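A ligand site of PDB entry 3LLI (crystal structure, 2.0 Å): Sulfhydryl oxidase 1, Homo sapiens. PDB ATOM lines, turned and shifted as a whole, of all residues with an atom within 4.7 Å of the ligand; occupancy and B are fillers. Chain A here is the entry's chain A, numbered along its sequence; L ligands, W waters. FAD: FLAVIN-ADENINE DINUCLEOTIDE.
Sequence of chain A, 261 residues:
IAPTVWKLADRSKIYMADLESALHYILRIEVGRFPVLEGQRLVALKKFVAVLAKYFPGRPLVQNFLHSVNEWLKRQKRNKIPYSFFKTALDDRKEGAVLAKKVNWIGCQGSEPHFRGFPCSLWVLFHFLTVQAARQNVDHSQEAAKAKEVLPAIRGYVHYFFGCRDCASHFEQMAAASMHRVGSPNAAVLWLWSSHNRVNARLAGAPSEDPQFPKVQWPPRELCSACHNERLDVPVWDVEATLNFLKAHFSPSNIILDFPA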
ATOM      1  N   ARG A  11     -19.097  39.418   3.979  1.00  0.00           N
ATOM      2  CA  ARG A  11     -19.747  38.119   3.831  1.00  0.00           C
ATOM      3  C   ARG A  11     -18.957  37.128   2.981  1.00  0.00           C
ATOM      4  O   ARG A  11     -19.110  35.915   3.123  1.00  0.00           O
ATOM      5  CB  ARG A  11     -21.151  38.284   3.233  1.00  0.00           C
ATOM      6  CG  ARG A  11     -22.208  38.757   4.219  1.00  0.00           C
ATOM      7  CD  ARG A  11     -23.550  38.952   3.525  1.00  0.00           C
ATOM      8  NE  ARG A  11     -24.649  39.168   4.475  1.00  0.00           N
ATOM      9  CZ  ARG A  11     -25.130  38.236   5.291  1.00  0.00           C
ATOM     10  NH1 ARG A  11     -24.620  37.013   5.289  1.00  0.00           N
ATOM     11  NH2 ARG A  11     -26.128  38.530   6.117  1.00  0.00           N
ATOM     12  N   ARG A 116     -25.964  34.329  16.666  1.00  0.00           N
ATOM     13  CA  ARG A 116     -24.763  33.869  15.981  1.00  0.00           C
ATOM     14  C   ARG A 116     -23.628  33.500  16.939  1.00  0.00           C
ATOM     15  O   ARG A 116     -23.795  32.629  17.787  1.00  0.00           O
ATOM     16  CB  ARG A 116     -24.320  34.951  14.980  1.00  0.00           C
ATOM     17  CG  ARG A 116     -25.499  35.548  14.199  1.00  0.00           C
ATOM     18  CD  ARG A 116     -25.060  36.516  13.109  1.00  0.00           C
ATOM     19  NE  ARG A 116     -24.350  35.828  12.038  1.00  0.00           N
ATOM     20  CZ  ARG A 116     -23.444  36.397  11.260  1.00  0.00           C
ATOM     21  NH1 ARG A 116     -23.129  37.673  11.449  1.00  0.00           N
ATOM     22  NH2 ARG A 116     -22.846  35.701  10.305  1.00  0.00           N
ATOM     23  N   PRO A 119     -21.770  29.095  17.297  1.00  0.00           N
ATOM     24  CA  PRO A 119     -22.389  28.205  16.316  1.00  0.00           C
ATOM     25  C   PRO A 119     -21.979  28.591  14.900  1.00  0.00           C
ATOM     26  O   PRO A 119     -21.666  27.749  14.056  1.00  0.00           O
ATOM     27  CB  PRO A 119     -23.883  28.416  16.544  1.00  0.00           C
ATOM     28  CG  PRO A 119     -23.945  28.664  18.017  1.00  0.00           C
ATOM     29  CD  PRO A 119     -22.794  29.626  18.233  1.00  0.00           C
ATOM     30  N   CYS A 120     -21.985  29.901  14.649  1.00  0.00           N
ATOM     31  CA  CYS A 120     -21.589  30.423  13.352  1.00  0.00           C
ATOM     32  C   CYS A 120     -20.125  30.091  13.097  1.00  0.00           C
ATOM     33  O   CYS A 120     -19.778  29.583  12.035  1.00  0.00           O
ATOM     34  CB  CYS A 120     -21.779  31.937  13.341  1.00  0.00           C
ATOM     35  SG  CYS A 120     -20.994  32.813  11.955  1.00  0.00           S
ATOM     36  N   LEU A 122     -18.415  27.723  14.363  1.00  0.00           N
ATOM     37  CA  LEU A 122     -18.233  26.277  14.266  1.00  0.00           C
ATOM     38  C   LEU A 122     -18.607  25.757  12.858  1.00  0.00           C
ATOM     39  O   LEU A 122     -17.949  24.861  12.351  1.00  0.00           O
ATOM     40  CB  LEU A 122     -19.057  25.539  15.331  1.00  0.00           C
ATOM     41  CG  LEU A 122     -18.837  24.027  15.502  1.00  0.00           C
ATOM     42  CD1 LEU A 122     -17.361  23.770  15.878  1.00  0.00           C
ATOM     43  CD2 LEU A 122     -19.767  23.453  16.598  1.00  0.00           C
ATOM     44  N   TRP A 123     -19.656  26.297  12.253  1.00  0.00           N
ATOM     45  CA  TRP A 123     -20.018  25.884  10.889  1.00  0.00           C
ATOM     46  C   TRP A 123     -18.832  26.275   9.977  1.00  0.00           C
ATOM     47  O   TRP A 123     -18.309  25.444   9.238  1.00  0.00           O
ATOM     48  CB  TRP A 123     -21.253  26.628  10.397  1.00  0.00           C
ATOM     49  CG  TRP A 123     -22.540  25.949  10.669  1.00  0.00           C
ATOM     50  CD1 TRP A 123     -23.602  26.471  11.339  1.00  0.00           C
ATOM     51  CD2 TRP A 123     -22.952  24.663  10.172  1.00  0.00           C
ATOM     52  NE1 TRP A 123     -24.666  25.596  11.279  1.00  0.00           N
ATOM     53  CE2 TRP A 123     -24.293  24.483  10.578  1.00  0.00           C
ATOM     54  CE3 TRP A 123     -22.315  23.657   9.437  1.00  0.00           C
ATOM     55  CZ2 TRP A 123     -25.015  23.326  10.249  1.00  0.00           C
ATOM     56  CZ3 TRP A 123     -23.038  22.500   9.108  1.00  0.00           C
ATOM     57  CH2 TRP A 123     -24.373  22.351   9.519  1.00  0.00           C
ATOM     58  N   VAL A 124     -18.425  27.535  10.047  1.00  0.00           N
ATOM     59  CA  VAL A 124     -17.301  28.024   9.233  1.00  0.00           C
ATOM     60  C   VAL A 124     -16.142  27.065   9.408  1.00  0.00           C
ATOM     61  O   VAL A 124     -15.606  26.564   8.426  1.00  0.00           O
ATOM     62  CB  VAL A 124     -16.884  29.462   9.638  1.00  0.00           C
ATOM     63  CG1 VAL A 124     -15.688  29.923   8.822  1.00  0.00           C
ATOM     64  CG2 VAL A 124     -18.064  30.417   9.438  1.00  0.00           C
ATOM     65  N   PHE A 126     -16.113  23.872  10.457  1.00  0.00           N
ATOM     66  CA  PHE A 126     -16.435  22.572   9.862  1.00  0.00           C
ATOM     67  C   PHE A 126     -16.277  22.616   8.323  1.00  0.00           C
ATOM     68  O   PHE A 126     -15.742  21.695   7.713  1.00  0.00           O
ATOM     69  CB  PHE A 126     -17.876  22.155  10.197  1.00  0.00           C
ATOM     70  CG  PHE A 126     -18.074  21.663  11.622  1.00  0.00           C
ATOM     71  CD1 PHE A 126     -17.002  21.284  12.425  1.00  0.00           C
ATOM     72  CD2 PHE A 126     -19.374  21.476  12.122  1.00  0.00           C
ATOM     73  CE1 PHE A 126     -17.211  20.718  13.704  1.00  0.00           C
ATOM     74  CE2 PHE A 126     -19.591  20.912  13.394  1.00  0.00           C
ATOM     75  CZ  PHE A 126     -18.510  20.539  14.189  1.00  0.00           C
ATOM     76  N   HIS A 127     -16.768  23.687   7.706  1.00  0.00           N
ATOM     77  CA  HIS A 127     -16.656  23.811   6.256  1.00  0.00           C
ATOM     78  C   HIS A 127     -15.186  23.896   5.850  1.00  0.00           C
ATOM     79  O   HIS A 127     -14.760  23.197   4.941  1.00  0.00           O
ATOM     80  CB  HIS A 127     -17.431  25.031   5.767  1.00  0.00           C
ATOM     81  CG  HIS A 127     -18.920  24.883   5.878  1.00  0.00           C
ATOM     82  ND1 HIS A 127     -19.611  23.871   5.262  1.00  0.00           N
ATOM     83  CD2 HIS A 127     -19.840  25.618   6.542  1.00  0.00           C
ATOM     84  CE1 HIS A 127     -20.903  23.983   5.528  1.00  0.00           C
ATOM     85  NE2 HIS A 127     -21.066  25.040   6.308  1.00  0.00           N
ATOM     86  N   VAL A 158     -19.855  16.959  17.242  1.00  0.00           N
ATOM     87  CA  VAL A 158     -21.180  17.532  17.441  1.00  0.00           C
ATOM     88  C   VAL A 158     -22.005  16.747  18.472  1.00  0.00           C
ATOM     89  O   VAL A 158     -22.676  17.335  19.327  1.00  0.00           O
ATOM     90  CB  VAL A 158     -21.970  17.557  16.138  1.00  0.00           C
ATOM     91  CG1 VAL A 158     -23.426  17.953  16.425  1.00  0.00           C
ATOM     92  CG2 VAL A 158     -21.343  18.535  15.164  1.00  0.00           C
ATOM     93  N   PHE A 162     -20.816  19.520  21.230  1.00  0.00           N
ATOM     94  CA  PHE A 162     -21.544  20.721  20.871  1.00  0.00           C
ATOM     95  C   PHE A 162     -22.639  21.093  21.879  1.00  0.00           C
ATOM     96  O   PHE A 162     -23.501  20.282  22.231  1.00  0.00           O
ATOM     97  CB  PHE A 162     -22.125  20.597  19.450  1.00  0.00           C
ATOM     98  CG  PHE A 162     -22.682  21.896  18.906  1.00  0.00           C
ATOM     99  CD1 PHE A 162     -22.140  23.112  19.315  1.00  0.00           C
ATOM    100  CD2 PHE A 162     -23.718  21.894  17.989  1.00  0.00           C
ATOM    101  CE1 PHE A 162     -22.649  24.309  18.818  1.00  0.00           C
ATOM    102  CE2 PHE A 162     -24.237  23.085  17.486  1.00  0.00           C
ATOM    103  CZ  PHE A 162     -23.702  24.303  17.904  1.00  0.00           C
ATOM    104  N   ASP A 166     -30.321  20.829  20.786  1.00  0.00           N
ATOM    105  CA  ASP A 166     -31.355  21.145  19.815  1.00  0.00           C
ATOM    106  C   ASP A 166     -30.666  21.131  18.452  1.00  0.00           C
ATOM    107  O   ASP A 166     -31.201  20.679  17.429  1.00  0.00           O
ATOM    108  CB  ASP A 166     -31.909  22.543  20.118  1.00  0.00           C
ATOM    109  CG  ASP A 166     -33.354  22.698  19.712  1.00  0.00           C
ATOM    110  OD1 ASP A 166     -34.164  21.798  20.030  1.00  0.00           O
ATOM    111  OD2 ASP A 166     -33.687  23.739  19.102  1.00  0.00           O
ATOM    112  N   CYS A 167     -29.439  21.646  18.480  1.00  0.00           N
ATOM    113  CA  CYS A 167     -28.621  21.738  17.295  1.00  0.00           C
ATOM    114  C   CYS A 167     -28.016  20.385  16.884  1.00  0.00           C
ATOM    115  O   CYS A 167     -28.070  20.007  15.711  1.00  0.00           O
ATOM    116  CB  CYS A 167     -27.508  22.763  17.551  1.00  0.00           C
ATOM    117  SG  CYS A 167     -28.069  24.406  18.139  1.00  0.00           S
ATOM    118  N   ALA A 168     -27.462  19.656  17.852  1.00  0.00           N
ATOM    119  CA  ALA A 168     -26.830  18.360  17.592  1.00  0.00           C
ATOM    120  C   ALA A 168     -27.821  17.301  17.141  1.00  0.00           C
ATOM    121  O   ALA A 168     -27.459  16.382  16.385  1.00  0.00           O
ATOM    122  CB  ALA A 168     -26.092  17.875  18.839  1.00  0.00           C
ATOM    123  N   HIS A 170     -30.552  17.797  15.285  1.00  0.00           N
ATOM    124  CA  HIS A 170     -30.882  18.049  13.887  1.00  0.00           C
ATOM    125  C   HIS A 170     -29.748  17.686  12.901  1.00  0.00           C
ATOM    126  O   HIS A 170     -30.021  17.290  11.760  1.00  0.00           O
ATOM    127  CB  HIS A 170     -31.312  19.513  13.676  1.00  0.00           C
ATOM    128  CG  HIS A 170     -32.671  19.819  14.232  1.00  0.00           C
ATOM    129  ND1 HIS A 170     -33.233  21.080  14.183  1.00  0.00           N
ATOM    130  CD2 HIS A 170     -33.594  19.023  14.827  1.00  0.00           C
ATOM    131  CE1 HIS A 170     -34.426  21.047  14.726  1.00  0.00           C
ATOM    132  NE2 HIS A 170     -34.678  19.812  15.127  1.00  0.00           N
ATOM    133  N   PHE A 171     -28.498  17.838  13.324  1.00  0.00           N
ATOM    134  CA  PHE A 171     -27.356  17.473  12.473  1.00  0.00           C
ATOM    135  C   PHE A 171     -27.309  15.962  12.368  1.00  0.00           C
ATOM    136  O   PHE A 171     -27.212  15.401  11.280  1.00  0.00           O
ATOM    137  CB  PHE A 171     -26.036  17.960  13.075  1.00  0.00           C
ATOM    138  CG  PHE A 171     -24.812  17.576  12.262  1.00  0.00           C
ATOM    139  CD1 PHE A 171     -24.366  18.382  11.213  1.00  0.00           C
ATOM    140  CD2 PHE A 171     -24.100  16.417  12.544  1.00  0.00           C
ATOM    141  CE1 PHE A 171     -23.225  18.038  10.469  1.00  0.00           C
ATOM    142  CE2 PHE A 171     -22.966  16.054  11.801  1.00  0.00           C
ATOM    143  CZ  PHE A 171     -22.522  16.872  10.758  1.00  0.00           C
ATOM    144  N   TRP A 193     -22.157  21.154   2.925  1.00  0.00           N
ATOM    145  CA  TRP A 193     -22.729  22.357   2.329  1.00  0.00           C
ATOM    146  C   TRP A 193     -24.260  22.283   2.229  1.00  0.00           C
ATOM    147  O   TRP A 193     -24.964  23.210   2.641  1.00  0.00           O
ATOM    148  CB  TRP A 193     -22.130  22.582   0.928  1.00  0.00           C
ATOM    149  CG  TRP A 193     -22.979  23.448   0.047  1.00  0.00           C
ATOM    150  CD1 TRP A 193     -23.246  24.782   0.204  1.00  0.00           C
ATOM    151  CD2 TRP A 193     -23.725  23.027  -1.096  1.00  0.00           C
ATOM    152  NE1 TRP A 193     -24.121  25.207  -0.772  1.00  0.00           N
ATOM    153  CE2 TRP A 193     -24.424  24.151  -1.585  1.00  0.00           C
ATOM    154  CE3 TRP A 193     -23.872  21.802  -1.762  1.00  0.00           C
ATOM    155  CZ2 TRP A 193     -25.261  24.081  -2.707  1.00  0.00           C
ATOM    156  CZ3 TRP A 193     -24.706  21.733  -2.870  1.00  0.00           C
ATOM    157  CH2 TRP A 193     -25.386  22.873  -3.326  1.00  0.00           C
ATOM    158  N   HIS A 196     -26.048  22.008   5.639  1.00  0.00           N
ATOM    159  CA  HIS A 196     -26.153  23.312   6.303  1.00  0.00           C
ATOM    160  C   HIS A 196     -27.315  24.103   5.691  1.00  0.00           C
ATOM    161  O   HIS A 196     -28.038  24.837   6.391  1.00  0.00           O
ATOM    162  CB  HIS A 196     -24.837  24.112   6.172  1.00  0.00           C
ATOM    163  CG  HIS A 196     -24.804  25.403   6.938  1.00  0.00           C
ATOM    164  ND1 HIS A 196     -23.631  26.098   7.168  1.00  0.00           N
ATOM    165  CD2 HIS A 196     -25.789  26.143   7.504  1.00  0.00           C
ATOM    166  CE1 HIS A 196     -23.900  27.210   7.840  1.00  0.00           C
ATOM    167  NE2 HIS A 196     -25.202  27.257   8.060  1.00  0.00           N
ATOM    168  N   ASN A 197     -27.502  23.949   4.380  1.00  0.00           N
ATOM    169  CA  ASN A 197     -28.601  24.644   3.719  1.00  0.00           C
ATOM    170  C   ASN A 197     -29.944  24.045   4.140  1.00  0.00           C
ATOM    171  O   ASN A 197     -30.940  24.748   4.136  1.00  0.00           O
ATOM    172  CB  ASN A 197     -28.457  24.609   2.199  1.00  0.00           C
ATOM    173  CG  ASN A 197     -27.703  25.813   1.664  1.00  0.00           C
ATOM    174  OD1 ASN A 197     -27.719  26.892   2.258  1.00  0.00           O
ATOM    175  ND2 ASN A 197     -27.052  25.640   0.512  1.00  0.00           N
ATOM    176  N   VAL A 199     -30.515  23.003   7.131  1.00  0.00           N
ATOM    177  CA  VAL A 199     -30.653  23.643   8.429  1.00  0.00           C
ATOM    178  C   VAL A 199     -31.087  25.084   8.198  1.00  0.00           C
ATOM    179  O   VAL A 199     -31.959  25.587   8.906  1.00  0.00           O
ATOM    180  CB  VAL A 199     -29.308  23.608   9.231  1.00  0.00           C
ATOM    181  CG1 VAL A 199     -29.408  24.458  10.503  1.00  0.00           C
ATOM    182  CG2 VAL A 199     -28.987  22.183   9.606  1.00  0.00           C
ATOM    183  N   ASN A 200     -30.506  25.754   7.206  1.00  0.00           N
ATOM    184  CA  ASN A 200     -30.893  27.127   6.906  1.00  0.00           C
ATOM    185  C   ASN A 200     -32.376  27.193   6.545  1.00  0.00           C
ATOM    186  O   ASN A 200     -33.082  28.128   6.913  1.00  0.00           O
ATOM    187  CB  ASN A 200     -30.047  27.719   5.757  1.00  0.00           C
ATOM    188  CG  ASN A 200     -28.561  27.846   6.112  1.00  0.00           C
ATOM    189  OD1 ASN A 200     -28.200  27.961   7.293  1.00  0.00           O
ATOM    190  ND2 ASN A 200     -27.701  27.839   5.096  1.00  0.00           N
ATOM    191  N   LEU A 203     -34.485  26.923   9.779  1.00  0.00           N
ATOM    192  CA  LEU A 203     -34.405  28.095  10.635  1.00  0.00           C
ATOM    193  C   LEU A 203     -34.849  29.408  10.024  1.00  0.00           C
ATOM    194  O   LEU A 203     -35.039  30.383  10.739  1.00  0.00           O
ATOM    195  CB  LEU A 203     -32.982  28.253  11.176  1.00  0.00           C
ATOM    196  CG  LEU A 203     -32.357  27.025  11.844  1.00  0.00           C
ATOM    197  CD1 LEU A 203     -30.962  27.399  12.375  1.00  0.00           C
ATOM    198  CD2 LEU A 203     -33.230  26.539  12.972  1.00  0.00           C
ATOM    199  N   SER A 208     -35.928  32.867  16.427  1.00  0.00           N
ATOM    200  CA  SER A 208     -34.567  32.877  16.968  1.00  0.00           C
ATOM    201  C   SER A 208     -33.546  33.401  15.968  1.00  0.00           C
ATOM    202  O   SER A 208     -32.370  33.586  16.301  1.00  0.00           O
ATOM    203  CB  SER A 208     -34.163  31.463  17.359  1.00  0.00           C
ATOM    204  OG  SER A 208     -34.135  30.621  16.212  1.00  0.00           O
ATOM    205  N   PHE A 213     -29.389  39.222  10.176  1.00  0.00           N
ATOM    206  CA  PHE A 213     -28.751  38.187   9.363  1.00  0.00           C
ATOM    207  C   PHE A 213     -29.678  37.033   8.992  1.00  0.00           C
ATOM    208  O   PHE A 213     -29.455  35.886   9.386  1.00  0.00           O
ATOM    209  CB  PHE A 213     -27.522  37.651  10.092  1.00  0.00           C
ATOM    210  CG  PHE A 213     -26.463  38.672  10.298  1.00  0.00           C
ATOM    211  CD1 PHE A 213     -25.604  39.020   9.263  1.00  0.00           C
ATOM    212  CD2 PHE A 213     -26.331  39.316  11.529  1.00  0.00           C
ATOM    213  CE1 PHE A 213     -24.633  39.987   9.440  1.00  0.00           C
ATOM    214  CE2 PHE A 213     -25.365  40.286  11.715  1.00  0.00           C
ATOM    215  CZ  PHE A 213     -24.501  40.631  10.671  1.00  0.00           C
ATOM    216  N   LYS A 215     -31.646  33.993   7.206  1.00  0.00           N
ATOM    217  CA  LYS A 215     -31.151  32.782   6.562  1.00  0.00           C
ATOM    218  C   LYS A 215     -31.547  32.785   5.096  1.00  0.00           C
ATOM    219  O   LYS A 215     -32.616  33.279   4.725  1.00  0.00           O
ATOM    220  CB  LYS A 215     -31.749  31.547   7.219  1.00  0.00           C
ATOM    221  CG  LYS A 215     -31.563  31.458   8.711  1.00  0.00           C
ATOM    222  CD  LYS A 215     -30.161  31.025   9.076  1.00  0.00           C
ATOM    223  CE  LYS A 215     -30.003  30.992  10.591  1.00  0.00           C
ATOM    224  NZ  LYS A 215     -28.849  30.154  10.998  1.00  0.00           N
ATOM    225  N   TRP A 218     -27.607  29.464   0.952  1.00  0.00           N
ATOM    226  CA  TRP A 218     -26.234  29.928   0.718  1.00  0.00           C
ATOM    227  C   TRP A 218     -25.427  29.049  -0.239  1.00  0.00           C
ATOM    228  O   TRP A 218     -25.514  27.822  -0.198  1.00  0.00           O
ATOM    229  CB  TRP A 218     -25.533  29.967   2.089  1.00  0.00           C
ATOM    230  CG  TRP A 218     -24.241  30.706   2.143  1.00  0.00           C
ATOM    231  CD1 TRP A 218     -24.046  31.988   2.578  1.00  0.00           C
ATOM    232  CD2 TRP A 218     -22.946  30.180   1.854  1.00  0.00           C
ATOM    233  NE1 TRP A 218     -22.703  32.291   2.576  1.00  0.00           N
ATOM    234  CE2 TRP A 218     -22.013  31.193   2.129  1.00  0.00           C
ATOM    235  CE3 TRP A 218     -22.487  28.945   1.374  1.00  0.00           C
ATOM    236  CZ2 TRP A 218     -20.623  31.016   1.943  1.00  0.00           C
ATOM    237  CZ3 TRP A 218     -21.114  28.764   1.191  1.00  0.00           C
ATOM    238  CH2 TRP A 218     -20.203  29.797   1.468  1.00  0.00           C
ATOM    239  N   LEU A 246     -16.844  27.120  -3.159  1.00  0.00           N
ATOM    240  CA  LEU A 246     -16.537  26.677  -1.808  1.00  0.00           C
ATOM    241  C   LEU A 246     -15.020  26.627  -1.594  1.00  0.00           C
ATOM    242  O   LEU A 246     -14.485  27.255  -0.663  1.00  0.00           O
ATOM    243  CB  LEU A 246     -17.166  25.300  -1.542  1.00  0.00           C
ATOM    244  CG  LEU A 246     -18.700  25.217  -1.512  1.00  0.00           C
ATOM    245  CD1 LEU A 246     -19.151  23.776  -1.391  1.00  0.00           C
ATOM    246  CD2 LEU A 246     -19.225  26.023  -0.343  1.00  0.00           C
ATOM    247  N   PHE A 250     -13.533  28.899   1.138  1.00  0.00           N
ATOM    248  CA  PHE A 250     -12.995  28.262   2.341  1.00  0.00           C
ATOM    249  C   PHE A 250     -11.557  27.861   2.042  1.00  0.00           C
ATOM    250  O   PHE A 250     -11.231  26.676   1.986  1.00  0.00           O
ATOM    251  CB  PHE A 250     -13.838  27.037   2.732  1.00  0.00           C
ATOM    252  CG  PHE A 250     -15.255  27.367   3.174  1.00  0.00           C
ATOM    253  CD1 PHE A 250     -15.487  28.077   4.355  1.00  0.00           C
ATOM    254  CD2 PHE A 250     -16.348  26.978   2.400  1.00  0.00           C
ATOM    255  CE1 PHE A 250     -16.795  28.403   4.759  1.00  0.00           C
ATOM    256  CE2 PHE A 250     -17.670  27.297   2.786  1.00  0.00           C
ATOM    257  CZ  PHE A 250     -17.890  28.015   3.972  1.00  0.00           C
HETATM  258  PA  FAD L   1     -24.736  30.213  10.243  1.00  0.00           P
HETATM  259  O1A FAD L   1     -24.109  30.008  11.575  1.00  0.00           O
HETATM  260  O2A FAD L   1     -25.792  29.322   9.696  1.00  0.00           O
HETATM  261  O5B FAD L   1     -23.629  30.325   9.137  1.00  0.00           O
HETATM  262  C5B FAD L   1     -22.263  30.692   9.344  1.00  0.00           C
HETATM  263  C4B FAD L   1     -21.906  31.348   8.033  1.00  0.00           C
HETATM  264  O4B FAD L   1     -21.426  30.255   7.195  1.00  0.00           O
HETATM  265  C3B FAD L   1     -22.727  32.371   7.215  1.00  0.00           C
HETATM  266  O3B FAD L   1     -22.672  33.722   7.668  1.00  0.00           O
HETATM  267  C2B FAD L   1     -22.224  32.088   5.873  1.00  0.00           C
HETATM  268  O2B FAD L   1     -21.093  32.810   5.501  1.00  0.00           O
HETATM  269  C1B FAD L   1     -21.855  30.598   5.872  1.00  0.00           C
HETATM  270  N9A FAD L   1     -22.814  29.633   5.421  1.00  0.00           N
HETATM  271  C8A FAD L   1     -24.233  29.619   5.403  1.00  0.00           C
HETATM  272  N7A FAD L   1     -24.797  28.586   4.883  1.00  0.00           N
HETATM  273  C5A FAD L   1     -23.690  27.824   4.501  1.00  0.00           C
HETATM  274  C6A FAD L   1     -23.638  26.595   3.835  1.00  0.00           C
HETATM  275  N6A FAD L   1     -24.723  25.932   3.413  1.00  0.00           N
HETATM  276  N1A FAD L   1     -22.420  26.022   3.524  1.00  0.00           N
HETATM  277  C2A FAD L   1     -21.230  26.637   3.782  1.00  0.00           C
HETATM  278  N3A FAD L   1     -21.273  27.873   4.439  1.00  0.00           N
HETATM  279  C4A FAD L   1     -22.544  28.417   4.788  1.00  0.00           C
HETATM  280  N1  FAD L   1     -29.972  26.317  15.644  1.00  0.00           N
HETATM  281  C2  FAD L   1     -31.318  26.161  15.935  1.00  0.00           C
HETATM  282  O2  FAD L   1     -31.919  27.166  16.350  1.00  0.00           O
HETATM  283  N3  FAD L   1     -31.737  24.865  15.653  1.00  0.00           N
HETATM  284  C4  FAD L   1     -30.977  23.787  15.146  1.00  0.00           C
HETATM  285  O4  FAD L   1     -31.519  22.639  14.992  1.00  0.00           O
HETATM  286  C4X FAD L   1     -29.644  24.049  14.896  1.00  0.00           C
HETATM  287  N5  FAD L   1     -28.763  22.996  14.478  1.00  0.00           N
HETATM  288  C5X FAD L   1     -27.362  23.152  14.315  1.00  0.00           C
HETATM  289  C6  FAD L   1     -26.593  22.014  14.015  1.00  0.00           C
HETATM  290  C7  FAD L   1     -25.198  22.182  13.831  1.00  0.00           C
HETATM  291  C7M FAD L   1     -24.421  20.899  13.514  1.00  0.00           C
HETATM  292  C8  FAD L   1     -24.589  23.472  13.928  1.00  0.00           C
HETATM  293  C8M FAD L   1     -23.134  23.863  13.728  1.00  0.00           C
HETATM  294  C9  FAD L   1     -25.380  24.567  14.254  1.00  0.00           C
HETATM  295  C9A FAD L   1     -26.772  24.492  14.520  1.00  0.00           C
HETATM  296  N10 FAD L   1     -27.801  25.511  14.861  1.00  0.00           N
HETATM  297  C10 FAD L   1     -29.130  25.359  15.149  1.00  0.00           C
HETATM  298  C1' FAD L   1     -27.369  26.864  14.759  1.00  0.00           C
HETATM  299  C2' FAD L   1     -27.524  27.585  13.449  1.00  0.00           C
HETATM  300  O2' FAD L   1     -27.251  26.691  12.340  1.00  0.00           O
HETATM  301  C3' FAD L   1     -26.728  28.834  13.220  1.00  0.00           C
HETATM  302  O3' FAD L   1     -25.352  28.570  13.440  1.00  0.00           O
HETATM  303  C4' FAD L   1     -27.134  30.132  13.905  1.00  0.00           C
HETATM  304  O4' FAD L   1     -28.581  30.291  13.892  1.00  0.00           O
HETATM  305  C5' FAD L   1     -26.466  31.371  13.488  1.00  0.00           C
HETATM  306  O5' FAD L   1     -26.851  31.607  12.134  1.00  0.00           O
HETATM  307  P   FAD L   1     -26.126  32.578  11.168  1.00  0.00           P
HETATM  308  O1P FAD L   1     -27.230  33.193  10.432  1.00  0.00           O
HETATM  309  O2P FAD L   1     -25.218  33.531  11.855  1.00  0.00           O
HETATM  310  O3P FAD L   1     -25.222  31.730  10.139  1.00  0.00           O
HETATM  311  O   HOH W   1     -29.795  28.818  15.854  1.00  0.00           O
HETATM  312  O   HOH W   2     -29.135  34.225  11.892  1.00  0.00           O
HETATM  313  O   HOH W   3     -31.337  25.368  18.874  1.00  0.00           O
HETATM  314  O   HOH W   4     -28.107  27.910   9.969  1.00  0.00           O
HETATM  315  O   HOH W   5     -26.704  30.792   7.102  1.00  0.00           O
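A ring nitrogen (ND1) of His 170 lies within hydrogen-bond range of an oxygen (O4) of the ligand (2.5 Å).
An oxygen (O2P) of the ligand is in salt-bridge range of the guanidinium group of Arg 116, at 2.5 Å.
NE2 of His 196 lies within hydrogen-bond range of O2A of the ligand (2.7 Å).
The side-chain amino group (NZ) of Lys 215 lies within salt-bridge range of an oxygen (O2A) of the ligand, 3.4 Å away.
The backbone carbonyl oxygen (O) of Trp 193 sits at hydrogen-bond distance from a nitrogen (N6A) of the ligand, at 2.8 Å.
NE2 of His 127 sits close to N1A of the ligand, 3.2 Å away.
The indole nitrogen (NE1) of Trp 123 is in hydrogen-bond range of an oxygen (O2') of the ligand (3.0 Å).
The side-chain amide nitrogen of Asn 200 is in hydrogen-bond range of a nitrogen (N7A) of the ligand (3.0 Å).
NE1 of Trp 218 lies close to O2B of the ligand, at 3.4 Å.
N6A of the ligand lies within hydrogen-bond range of OD1 of Asn 197 (3.4 Å).
Water W2 bridges an oxygen (O1P) of the ligand (2.6 Å) and the backbone carbonyl oxygen (O) of Phe 213 (3.0 Å).
Water W4 lies within hydrogen-bond range of NZ of Lys 215 (2.6 Å), OD1 of Asn 200 (2.7 Å) and O2A of the ligand (2.7 Å).
Water W5 bridges O2A of the ligand (3.1 Å) and OD1 of Asn 200 (3.2 Å).
A ring nitrogen (NE2) of His 127 is in hydrogen-bond range of a ring nitrogen (ND1) of His 196 (2.9 Å).
NE2 of His 196 lies close to OD1 of Asn 200 (3.2 Å).
The indole nitrogen of Trp 193 sits at hydrogen-bond distance from the backbone carbonyl oxygen of Trp 218, at 3.0 Å.
The indole nitrogen (NE1) of Trp 193 sits close to the side-chain amide nitrogen (ND2) of Asn 197, 3.2 Å away.
ND2 of Asn 200 sits at hydrogen-bond distance from OD1 of Asn 197 (3.0 Å).
The backbone carbonyl oxygen of Trp 218 lies within hydrogen-bond range of the side-chain amide nitrogen of Asn 197 (2.8 Å).
The backbone carbonyl oxygen of Asp 166 lies close to an oxygen (O4) of the ligand.
O of Cys 167 lies close to N5 of the ligand.
Pro 119 touches the ligand (CB to O3', 3.4 Å).
Cys 120 touches the ligand (CA to O1A, 3.1 Å).
Phe 162 touches the ligand.
CB of Phe 171 touches C7M of the ligand, at 3.4 Å.
Val 199 touches the ligand.
Leu 203 touches the ligand (CD2 to N3, 3.5 Å).
Phe 213 touches the ligand (O to O1P, 3.6 Å).
Phe 250 touches the ligand (CZ to N3A, 3.4 Å).
Hydrophobic or aromatic side chains that line the ligand: Pro 119, Trp 123, His 127, Phe 162, His 170, Phe 171, Trp 193, His 196, Val 199, Leu 203, Trp 218 and Phe 250.
Of the 28 residues printed, 20 come within 4 Å of the ligand.
Along chain A the residues within 4 Å of the ligand span positions 116 to 250.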
